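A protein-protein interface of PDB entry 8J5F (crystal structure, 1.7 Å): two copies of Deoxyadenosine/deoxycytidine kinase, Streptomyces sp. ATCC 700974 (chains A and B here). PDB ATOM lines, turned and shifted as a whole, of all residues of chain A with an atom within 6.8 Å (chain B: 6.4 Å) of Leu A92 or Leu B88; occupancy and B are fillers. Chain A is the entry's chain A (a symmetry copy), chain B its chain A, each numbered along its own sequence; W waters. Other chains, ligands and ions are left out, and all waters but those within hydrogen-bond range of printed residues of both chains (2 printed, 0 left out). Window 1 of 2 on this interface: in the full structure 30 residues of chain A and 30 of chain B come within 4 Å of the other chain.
A ring nitrogen (NE2) of His B69 sits at hydrogen-bond distance from the side-chain carboxylate (OE1) of Glu A93, 2.7 Å away.
The backbone carbonyl oxygen (O) of Leu A146 lies close to a ring nitrogen (ND1) of His A95, at 3.4 Å.
Among the printed residues, pairs that only touch across the chains: Leu A96 with His B69, Val A142 with Ala B138, Val A142 with Val B142, Leu A92 with Ser B89, Ser A89 with Leu B92, Leu A92 with Pro B85, Leu A146 with Phe B84, Leu A96 with Pro B85, Leu A92 with Leu B88, Leu A88 with Leu B92, Leu A88 with Val B142, Val A142 with Leu B88, Glu A93 with Glu B93 and His A95 with Pro B85.
Leu A92 touches just these residues of chain B: Pro B85, Leu B88 and Ser B89.
Printed residues of chain A within 4 Å of His B69: Glu A93 (2.7 Å) and Leu A96 (3.4 Å).
Of chain A, only Leu A92 (3.8 Å) and Val A142 (3.8 Å) come within 4 Å of Leu B88.
Met B91 touches none of the printed residues of chain A.
Tyr B139 touches none of the printed residues of chain A.
Printed residues of chain A within 4 Å of Val B142: Leu A88 (3.8 Å) and Val A142 (3.4 Å).
Of the 15 printed residues of chain A, 8 touch a printed residue of chain B.
Hydrophobic or aromatic side chains of chain A that line the printed part of chain B: Leu A88, Leu A92, His A95, Leu A96, Val A142 and Leu A146.
Along chain B the printed residues that touch a printed residue of chain A span positions 69 to 142.
Among the printed residues, no Asp or Glu carboxylate lies within 4 Å of a Lys or Arg side-chain nitrogen of the other chain.
Leu A88 touches Leu B92, and with the chains exchanged Leu A92 touches Leu B88.
Leu A88 touches Val B142, and with the chains exchanged Val A142 touches Leu B88.
Glu B93 touches its own counterpart, Glu A93.
Val B142 touches its own counterpart, Val A142.
Water W2 lies within hydrogen-bond range of OG of Ser B89, OE2 of Glu A93 and OE2 of Glu B93.
Water W1 lies within hydrogen-bond range of OG of Ser A89 (2.6 Å), OE2 of Glu B93 (2.6 Å) and OE2 of Glu A93 (2.7 Å).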
ATOM      1  N   PHE A  67     -35.952 -29.691  18.947  1.00  0.00           N
ATOM      2  CA  PHE A  67     -35.385 -28.350  18.873  1.00  0.00           C
ATOM      3  C   PHE A  67     -35.090 -27.907  17.440  1.00  0.00           C
ATOM      4  O   PHE A  67     -34.409 -26.892  17.251  1.00  0.00           O
ATOM      5  CB  PHE A  67     -34.130 -28.217  19.756  1.00  0.00           C
ATOM      6  CG  PHE A  67     -33.045 -29.252  19.516  1.00  0.00           C
ATOM      7  CD1 PHE A  67     -33.011 -30.436  20.238  1.00  0.00           C
ATOM      8  CD2 PHE A  67     -32.018 -28.999  18.621  1.00  0.00           C
ATOM      9  CE1 PHE A  67     -31.992 -31.370  20.042  1.00  0.00           C
ATOM     10  CE2 PHE A  67     -30.990 -29.924  18.422  1.00  0.00           C
ATOM     11  CZ  PHE A  67     -30.981 -31.112  19.134  1.00  0.00           C
ATOM     12  N   GLN A  87     -26.951 -24.220  11.268  1.00  0.00           N
ATOM     13  CA  GLN A  87     -25.987 -25.077  11.969  1.00  0.00           C
ATOM     14  C   GLN A  87     -25.642 -24.521  13.348  1.00  0.00           C
ATOM     15  O   GLN A  87     -25.471 -25.286  14.318  1.00  0.00           O
ATOM     16  CB  GLN A  87     -24.716 -25.258  11.142  1.00  0.00           C
ATOM     17  CG  GLN A  87     -24.901 -26.217   9.964  1.00  0.00           C
ATOM     18  CD  GLN A  87     -25.332 -27.609  10.401  1.00  0.00           C
ATOM     19  OE1 GLN A  87     -24.887 -28.126  11.432  1.00  0.00           O
ATOM     20  NE2 GLN A  87     -26.207 -28.226   9.611  1.00  0.00           N
ATOM     21  N   LEU A  88     -25.527 -23.195  13.464  1.00  0.00           N
ATOM     22  CA  LEU A  88     -25.339 -22.622  14.792  1.00  0.00           C
ATOM     23  C   LEU A  88     -26.517 -22.984  15.694  1.00  0.00           C
ATOM     24  O   LEU A  88     -26.330 -23.278  16.881  1.00  0.00           O
ATOM     25  CB  LEU A  88     -25.169 -21.097  14.708  1.00  0.00           C
ATOM     26  CG  LEU A  88     -23.855 -20.549  14.129  1.00  0.00           C
ATOM     27  CD1 LEU A  88     -24.028 -19.074  13.786  1.00  0.00           C
ATOM     28  CD2 LEU A  88     -22.663 -20.747  15.081  1.00  0.00           C
ATOM     29  N   SER A  89     -27.736 -22.996  15.138  1.00  0.00           N
ATOM     30  CA  SER A  89     -28.921 -23.329  15.924  1.00  0.00           C
ATOM     31  C   SER A  89     -28.867 -24.760  16.451  1.00  0.00           C
ATOM     32  O   SER A  89     -29.125 -24.997  17.638  1.00  0.00           O
ATOM     33  CB  SER A  89     -30.197 -23.120  15.103  1.00  0.00           C
ATOM     34  OG  SER A  89     -31.331 -23.533  15.857  1.00  0.00           O
ATOM     35  N   PHE A  90     -28.564 -25.734  15.580  1.00  0.00           N
ATOM     36  CA  PHE A  90     -28.455 -27.120  16.043  1.00  0.00           C
ATOM     37  C   PHE A  90     -27.475 -27.235  17.212  1.00  0.00           C
ATOM     38  O   PHE A  90     -27.808 -27.802  18.264  1.00  0.00           O
ATOM     39  CB  PHE A  90     -27.999 -28.036  14.902  1.00  0.00           C
ATOM     40  CG  PHE A  90     -29.123 -28.635  14.074  1.00  0.00           C
ATOM     41  CD1 PHE A  90     -29.890 -29.689  14.562  1.00  0.00           C
ATOM     42  CD2 PHE A  90     -29.356 -28.199  12.779  1.00  0.00           C
ATOM     43  CE1 PHE A  90     -30.892 -30.250  13.801  1.00  0.00           C
ATOM     44  CE2 PHE A  90     -30.352 -28.775  11.993  1.00  0.00           C
ATOM     45  CZ  PHE A  90     -31.126 -29.803  12.505  1.00  0.00           C
ATOM     46  N   MET A  91     -26.242 -26.740  17.016  1.00  0.00           N
ATOM     47  CA  MET A  91     -25.231 -26.693  18.077  1.00  0.00           C
ATOM     48  C   MET A  91     -25.771 -26.108  19.374  1.00  0.00           C
ATOM     49  O   MET A  91     -25.597 -26.677  20.461  1.00  0.00           O
ATOM     50  CB  MET A  91     -24.069 -25.814  17.653  1.00  0.00           C
ATOM     51  CG  MET A  91     -22.973 -25.729  18.708  1.00  0.00           C
ATOM     52  SD  MET A  91     -21.431 -25.090  18.043  1.00  0.00           S
ATOM     53  CE  MET A  91     -21.969 -23.425  17.632  1.00  0.00           C
ATOM     54  N   LEU A  92     -26.307 -24.892  19.279  1.00  0.00           N
ATOM     55  CA  LEU A  92     -26.650 -24.116  20.463  1.00  0.00           C
ATOM     56  C   LEU A  92     -27.813 -24.739  21.223  1.00  0.00           C
ATOM     57  O   LEU A  92     -27.777 -24.826  22.457  1.00  0.00           O
ATOM     58  CB  LEU A  92     -26.993 -22.683  20.064  1.00  0.00           C
ATOM     59  CG  LEU A  92     -27.401 -21.774  21.209  1.00  0.00           C
ATOM     60  CD1 LEU A  92     -26.273 -21.678  22.204  1.00  0.00           C
ATOM     61  CD2 LEU A  92     -27.754 -20.416  20.628  1.00  0.00           C
ATOM     62  N   GLU A  93     -28.859 -25.168  20.512  1.00  0.00           N
ATOM     63  CA  GLU A  93     -30.012 -25.763  21.183  1.00  0.00           C
ATOM     64  C   GLU A  93     -29.644 -27.099  21.823  1.00  0.00           C
ATOM     65  O   GLU A  93     -30.086 -27.399  22.942  1.00  0.00           O
ATOM     66  CB  GLU A  93     -31.168 -25.960  20.203  1.00  0.00           C
ATOM     67  CG  GLU A  93     -31.730 -24.683  19.592  1.00  0.00           C
ATOM     68  CD  GLU A  93     -32.281 -23.703  20.633  1.00  0.00           C
ATOM     69  OE1 GLU A  93     -32.674 -24.133  21.744  1.00  0.00           O
ATOM     70  OE2 GLU A  93     -32.327 -22.492  20.325  1.00  0.00           O
ATOM     71  N   ARG A  94     -28.841 -27.912  21.127  1.00  0.00           N
ATOM     72  CA  ARG A  94     -28.324 -29.137  21.738  1.00  0.00           C
ATOM     73  C   ARG A  94     -27.519 -28.823  22.994  1.00  0.00           C
ATOM     74  O   ARG A  94     -27.696 -29.465  24.043  1.00  0.00           O
ATOM     75  CB  ARG A  94     -27.458 -29.907  20.741  1.00  0.00           C
ATOM     76  CG  ARG A  94     -27.128 -31.318  21.218  1.00  0.00           C
ATOM     77  CD  ARG A  94     -26.003 -31.952  20.400  1.00  0.00           C
ATOM     78  NE  ARG A  94     -26.315 -31.978  18.974  1.00  0.00           N
ATOM     79  CZ  ARG A  94     -27.142 -32.833  18.390  1.00  0.00           C
ATOM     80  NH1 ARG A  94     -27.814 -33.738  19.089  1.00  0.00           N
ATOM     81  NH2 ARG A  94     -27.276 -32.799  17.067  1.00  0.00           N
ATOM     82  N   HIS A  95     -26.614 -27.839  22.898  1.00  0.00           N
ATOM     83  CA  HIS A  95     -25.774 -27.476  24.042  1.00  0.00           C
ATOM     84  C   HIS A  95     -26.619 -27.117  25.259  1.00  0.00           C
ATOM     85  O   HIS A  95     -26.347 -27.572  26.375  1.00  0.00           O
ATOM     86  CB  HIS A  95     -24.863 -26.295  23.686  1.00  0.00           C
ATOM     87  CG  HIS A  95     -24.091 -25.772  24.861  1.00  0.00           C
ATOM     88  ND1 HIS A  95     -22.912 -26.350  25.290  1.00  0.00           N
ATOM     89  CD2 HIS A  95     -24.341 -24.749  25.713  1.00  0.00           C
ATOM     90  CE1 HIS A  95     -22.464 -25.692  26.347  1.00  0.00           C
ATOM     91  NE2 HIS A  95     -23.317 -24.725  26.630  1.00  0.00           N
ATOM     92  N   LEU A  96     -27.627 -26.266  25.059  1.00  0.00           N
ATOM     93  CA  LEU A  96     -28.444 -25.781  26.172  1.00  0.00           C
ATOM     94  C   LEU A  96     -29.199 -26.925  26.844  1.00  0.00           C
ATOM     95  O   LEU A  96     -29.278 -26.990  28.082  1.00  0.00           O
ATOM     96  CB  LEU A  96     -29.413 -24.699  25.672  1.00  0.00           C
ATOM     97  CG  LEU A  96     -28.807 -23.297  25.558  1.00  0.00           C
ATOM     98  CD1 LEU A  96     -29.702 -22.374  24.723  1.00  0.00           C
ATOM     99  CD2 LEU A  96     -28.566 -22.705  26.949  1.00  0.00           C
ATOM    100  N   LEU A  97     -29.756 -27.843  26.047  1.00  0.00           N
ATOM    101  CA  LEU A  97     -30.433 -29.007  26.619  1.00  0.00           C
ATOM    102  C   LEU A  97     -29.470 -29.853  27.448  1.00  0.00           C
ATOM    103  O   LEU A  97     -29.834 -30.360  28.525  1.00  0.00           O
ATOM    104  CB  LEU A  97     -31.065 -29.852  25.501  1.00  0.00           C
ATOM    105  CG  LEU A  97     -32.439 -29.367  25.023  1.00  0.00           C
ATOM    106  CD1 LEU A  97     -32.773 -29.931  23.641  1.00  0.00           C
ATOM    107  CD2 LEU A  97     -33.548 -29.693  26.019  1.00  0.00           C
ATOM    108  N   ASP A 118     -22.026 -32.603  15.399  1.00  0.00           N
ATOM    109  CA  ASP A 118     -22.511 -31.459  14.621  1.00  0.00           C
ATOM    110  C   ASP A 118     -21.438 -30.900  13.699  1.00  0.00           C
ATOM    111  O   ASP A 118     -21.758 -30.392  12.617  1.00  0.00           O
ATOM    112  CB  ASP A 118     -23.036 -30.352  15.552  1.00  0.00           C
ATOM    113  CG  ASP A 118     -24.354 -30.716  16.218  1.00  0.00           C
ATOM    114  OD1 ASP A 118     -25.233 -31.290  15.541  1.00  0.00           O
ATOM    115  OD2 ASP A 118     -24.515 -30.425  17.424  1.00  0.00           O
ATOM    116  N   VAL A 142     -16.714 -20.932  18.673  1.00  0.00           N
ATOM    117  CA  VAL A 142     -17.838 -21.056  19.596  1.00  0.00           C
ATOM    118  C   VAL A 142     -18.020 -22.507  20.021  1.00  0.00           C
ATOM    119  O   VAL A 142     -18.175 -22.806  21.211  1.00  0.00           O
ATOM    120  CB  VAL A 142     -19.119 -20.482  18.967  1.00  0.00           C
ATOM    121  CG1 VAL A 142     -20.339 -20.879  19.799  1.00  0.00           C
ATOM    122  CG2 VAL A 142     -19.005 -18.961  18.920  1.00  0.00           C
ATOM    123  N   LEU A 146     -18.232 -24.016  23.840  1.00  0.00           N
ATOM    124  CA  LEU A 146     -19.429 -24.700  24.324  1.00  0.00           C
ATOM    125  C   LEU A 146     -19.113 -26.135  24.735  1.00  0.00           C
ATOM    126  O   LEU A 146     -19.527 -26.592  25.811  1.00  0.00           O
ATOM    127  CB  LEU A 146     -20.513 -24.693  23.248  1.00  0.00           C
ATOM    128  CG  LEU A 146     -21.118 -23.338  22.871  1.00  0.00           C
ATOM    129  CD1 LEU A 146     -22.103 -23.538  21.716  1.00  0.00           C
ATOM    130  CD2 LEU A 146     -21.834 -22.706  24.073  1.00  0.00           C
ATOM    131  N   HIS B  69     -35.614 -17.315  24.672  1.00  0.00           N
ATOM    132  CA  HIS B  69     -35.375 -18.733  24.907  1.00  0.00           C
ATOM    133  C   HIS B  69     -36.138 -19.229  26.135  1.00  0.00           C
ATOM    134  O   HIS B  69     -36.318 -18.512  27.124  1.00  0.00           O
ATOM    135  CB  HIS B  69     -33.884 -19.016  25.079  1.00  0.00           C
ATOM    136  CG  HIS B  69     -33.518 -20.418  24.730  1.00  0.00           C
ATOM    137  ND1 HIS B  69     -33.701 -21.472  25.600  1.00  0.00           N
ATOM    138  CD2 HIS B  69     -33.066 -20.954  23.574  1.00  0.00           C
ATOM    139  CE1 HIS B  69     -33.346 -22.595  25.003  1.00  0.00           C
ATOM    140  NE2 HIS B  69     -32.971 -22.309  23.768  1.00  0.00           N
ATOM    141  N   ALA B  83     -25.184 -17.362  30.719  1.00  0.00           N
ATOM    142  CA  ALA B  83     -25.145 -16.075  30.016  1.00  0.00           C
ATOM    143  C   ALA B  83     -24.573 -16.217  28.604  1.00  0.00           C
ATOM    144  O   ALA B  83     -25.115 -15.651  27.647  1.00  0.00           O
ATOM    145  CB  ALA B  83     -24.339 -15.051  30.813  1.00  0.00           C
ATOM    146  N   PHE B  84     -23.487 -16.986  28.446  1.00  0.00           N
ATOM    147  CA  PHE B  84     -22.889 -17.130  27.122  1.00  0.00           C
ATOM    148  C   PHE B  84     -23.848 -17.770  26.129  1.00  0.00           C
ATOM    149  O   PHE B  84     -24.102 -17.158  25.080  1.00  0.00           O
ATOM    150  CB  PHE B  84     -21.575 -17.915  27.224  1.00  0.00           C
ATOM    151  CG  PHE B  84     -20.876 -18.141  25.913  1.00  0.00           C
ATOM    152  CD1 PHE B  84     -20.604 -17.093  25.045  1.00  0.00           C
ATOM    153  CD2 PHE B  84     -20.486 -19.426  25.548  1.00  0.00           C
ATOM    154  CE1 PHE B  84     -19.941 -17.320  23.849  1.00  0.00           C
ATOM    155  CE2 PHE B  84     -19.830 -19.667  24.356  1.00  0.00           C
ATOM    156  CZ  PHE B  84     -19.550 -18.605  23.503  1.00  0.00           C
ATOM    157  N   PRO B  85     -24.429 -18.953  26.381  1.00  0.00           N
ATOM    158  CA  PRO B  85     -25.308 -19.525  25.346  1.00  0.00           C
ATOM    159  C   PRO B  85     -26.618 -18.771  25.183  1.00  0.00           C
ATOM    160  O   PRO B  85     -27.157 -18.756  24.076  1.00  0.00           O
ATOM    161  CB  PRO B  85     -25.543 -20.963  25.816  1.00  0.00           C
ATOM    162  CG  PRO B  85     -25.199 -20.975  27.277  1.00  0.00           C
ATOM    163  CD  PRO B  85     -24.121 -19.943  27.435  1.00  0.00           C
ATOM    164  N   ILE B  86     -27.157 -18.152  26.236  1.00  0.00           N
ATOM    165  CA  ILE B  86     -28.386 -17.383  26.043  1.00  0.00           C
ATOM    166  C   ILE B  86     -28.104 -16.107  25.241  1.00  0.00           C
ATOM    167  O   ILE B  86     -28.931 -15.685  24.423  1.00  0.00           O
ATOM    168  CB  ILE B  86     -29.063 -17.077  27.389  1.00  0.00           C
ATOM    169  CG1 ILE B  86     -29.512 -18.375  28.072  1.00  0.00           C
ATOM    170  CG2 ILE B  86     -30.287 -16.143  27.168  1.00  0.00           C
ATOM    171  CD1 ILE B  86     -30.523 -19.168  27.262  1.00  0.00           C
ATOM    172  N   GLN B  87     -26.931 -15.488  25.431  1.00  0.00           N
ATOM    173  CA  GLN B  87     -26.580 -14.360  24.561  1.00  0.00           C
ATOM    174  C   GLN B  87     -26.392 -14.805  23.114  1.00  0.00           C
ATOM    175  O   GLN B  87     -26.773 -14.085  22.171  1.00  0.00           O
ATOM    176  CB  GLN B  87     -25.320 -13.657  25.063  1.00  0.00           C
ATOM    177  CG  GLN B  87     -25.573 -12.787  26.297  1.00  0.00           C
ATOM    178  CD  GLN B  87     -26.605 -11.697  26.048  1.00  0.00           C
ATOM    179  OE1 GLN B  87     -26.661 -11.101  24.967  1.00  0.00           O
ATOM    180  NE2 GLN B  87     -27.430 -11.432  27.057  1.00  0.00           N
ATOM    181  N   LEU B  88     -25.800 -15.986  22.907  1.00  0.00           N
ATOM    182  CA  LEU B  88     -25.733 -16.506  21.546  1.00  0.00           C
ATOM    183  C   LEU B  88     -27.140 -16.678  20.976  1.00  0.00           C
ATOM    184  O   LEU B  88     -27.377 -16.394  19.796  1.00  0.00           O
ATOM    185  CB  LEU B  88     -24.967 -17.838  21.510  1.00  0.00           C
ATOM    186  CG  LEU B  88     -23.445 -17.801  21.724  1.00  0.00           C
ATOM    187  CD1 LEU B  88     -22.940 -19.207  22.024  1.00  0.00           C
ATOM    188  CD2 LEU B  88     -22.695 -17.201  20.522  1.00  0.00           C
ATOM    189  N   SER B  89     -28.092 -17.115  21.812  1.00  0.00           N
ATOM    190  CA  SER B  89     -29.466 -17.309  21.355  1.00  0.00           C
ATOM    191  C   SER B  89     -30.103 -15.999  20.904  1.00  0.00           C
ATOM    192  O   SER B  89     -30.713 -15.942  19.828  1.00  0.00           O
ATOM    193  CB  SER B  89     -30.318 -17.958  22.450  1.00  0.00           C
ATOM    194  OG  SER B  89     -31.669 -18.058  22.016  1.00  0.00           O
ATOM    195  N   PHE B  90     -30.002 -14.941  21.722  1.00  0.00           N
ATOM    196  CA  PHE B  90     -30.558 -13.648  21.317  1.00  0.00           C
ATOM    197  C   PHE B  90     -30.016 -13.218  19.952  1.00  0.00           C
ATOM    198  O   PHE B  90     -30.789 -12.880  19.043  1.00  0.00           O
ATOM    199  CB  PHE B  90     -30.233 -12.571  22.358  1.00  0.00           C
ATOM    200  CG  PHE B  90     -31.264 -12.417  23.462  1.00  0.00           C
ATOM    201  CD1 PHE B  90     -32.475 -11.771  23.229  1.00  0.00           C
ATOM    202  CD2 PHE B  90     -30.986 -12.843  24.752  1.00  0.00           C
ATOM    203  CE1 PHE B  90     -33.399 -11.607  24.238  1.00  0.00           C
ATOM    204  CE2 PHE B  90     -31.904 -12.662  25.784  1.00  0.00           C
ATOM    205  CZ  PHE B  90     -33.118 -12.045  25.528  1.00  0.00           C
ATOM    206  N   MET B  91     -28.680 -13.183  19.817  1.00  0.00           N
ATOM    207  CA  MET B  91     -28.022 -12.885  18.542  1.00  0.00           C
ATOM    208  C   MET B  91     -28.589 -13.699  17.387  1.00  0.00           C
ATOM    209  O   MET B  91     -28.920 -13.163  16.321  1.00  0.00           O
ATOM    210  CB  MET B  91     -26.545 -13.219  18.626  1.00  0.00           C
ATOM    211  CG  MET B  91     -25.794 -12.924  17.333  1.00  0.00           C
ATOM    212  SD  MET B  91     -24.014 -12.876  17.571  1.00  0.00           S
ATOM    213  CE  MET B  91     -23.742 -14.596  18.016  1.00  0.00           C
ATOM    214  N   LEU B  92     -28.568 -15.021  17.549  1.00  0.00           N
ATOM    215  CA  LEU B  92     -28.857 -15.928  16.446  1.00  0.00           C
ATOM    216  C   LEU B  92     -30.318 -15.847  16.023  1.00  0.00           C
ATOM    217  O   LEU B  92     -30.620 -15.815  14.823  1.00  0.00           O
ATOM    218  CB  LEU B  92     -28.506 -17.360  16.843  1.00  0.00           C
ATOM    219  CG  LEU B  92     -28.793 -18.412  15.788  1.00  0.00           C
ATOM    220  CD1 LEU B  92     -27.996 -18.110  14.546  1.00  0.00           C
ATOM    221  CD2 LEU B  92     -28.435 -19.768  16.368  1.00  0.00           C
ATOM    222  N   GLU B  93     -31.242 -15.825  16.988  1.00  0.00           N
ATOM    223  CA  GLU B  93     -32.661 -15.761  16.648  1.00  0.00           C
ATOM    224  C   GLU B  93     -33.010 -14.421  16.006  1.00  0.00           C
ATOM    225  O   GLU B  93     -33.792 -14.374  15.044  1.00  0.00           O
ATOM    226  CB  GLU B  93     -33.527 -15.981  17.887  1.00  0.00           C
ATOM    227  CG  GLU B  93     -33.379 -17.344  18.553  1.00  0.00           C
ATOM    228  CD  GLU B  93     -33.739 -18.512  17.628  1.00  0.00           C
ATOM    229  OE1 GLU B  93     -34.526 -18.325  16.669  1.00  0.00           O
ATOM    230  OE2 GLU B  93     -33.233 -19.627  17.877  1.00  0.00           O
ATOM    231  N   VAL B 122     -23.422  -8.662  26.014  1.00  0.00           N
ATOM    232  CA  VAL B 122     -22.264  -9.510  26.303  1.00  0.00           C
ATOM    233  C   VAL B 122     -21.216  -8.730  27.099  1.00  0.00           C
ATOM    234  O   VAL B 122     -20.593  -9.272  28.020  1.00  0.00           O
ATOM    235  CB  VAL B 122     -21.698 -10.094  24.997  1.00  0.00           C
ATOM    236  CG1 VAL B 122     -20.327 -10.726  25.231  1.00  0.00           C
ATOM    237  CG2 VAL B 122     -22.681 -11.125  24.468  1.00  0.00           C
ATOM    238  N   ALA B 138     -15.061 -15.571  21.034  1.00  0.00           N
ATOM    239  CA  ALA B 138     -15.780 -16.493  20.154  1.00  0.00           C
ATOM    240  C   ALA B 138     -17.101 -15.888  19.700  1.00  0.00           C
ATOM    241  O   ALA B 138     -17.446 -15.939  18.515  1.00  0.00           O
ATOM    242  CB  ALA B 138     -16.014 -17.828  20.874  1.00  0.00           C
ATOM    243  N   TYR B 139     -17.855 -15.313  20.642  1.00  0.00           N
ATOM    244  CA  TYR B 139     -19.086 -14.594  20.309  1.00  0.00           C
ATOM    245  C   TYR B 139     -18.833 -13.547  19.231  1.00  0.00           C
ATOM    246  O   TYR B 139     -19.572 -13.457  18.240  1.00  0.00           O
ATOM    247  CB  TYR B 139     -19.654 -13.944  21.584  1.00  0.00           C
ATOM    248  CG  TYR B 139     -20.872 -13.064  21.368  1.00  0.00           C
ATOM    249  CD1 TYR B 139     -20.728 -11.722  21.042  1.00  0.00           C
ATOM    250  CD2 TYR B 139     -22.164 -13.578  21.482  1.00  0.00           C
ATOM    251  CE1 TYR B 139     -21.832 -10.913  20.845  1.00  0.00           C
ATOM    252  CE2 TYR B 139     -23.289 -12.769  21.293  1.00  0.00           C
ATOM    253  CZ  TYR B 139     -23.107 -11.437  20.970  1.00  0.00           C
ATOM    254  OH  TYR B 139     -24.180 -10.602  20.766  1.00  0.00           O
ATOM    255  N   VAL B 142     -18.355 -14.892  15.606  1.00  0.00           N
ATOM    256  CA  VAL B 142     -19.627 -15.262  14.991  1.00  0.00           C
ATOM    257  C   VAL B 142     -20.458 -14.020  14.696  1.00  0.00           C
ATOM    258  O   VAL B 142     -21.001 -13.865  13.596  1.00  0.00           O
ATOM    259  CB  VAL B 142     -20.388 -16.258  15.883  1.00  0.00           C
ATOM    260  CG1 VAL B 142     -21.829 -16.411  15.393  1.00  0.00           C
ATOM    261  CG2 VAL B 142     -19.682 -17.610  15.825  1.00  0.00           C
HETATM  262  O   HOH W   1     -31.896 -21.882  17.731  1.00  0.00           O
HETATM  263  O   HOH W   2     -31.983 -19.891  20.254  1.00  0.00           O
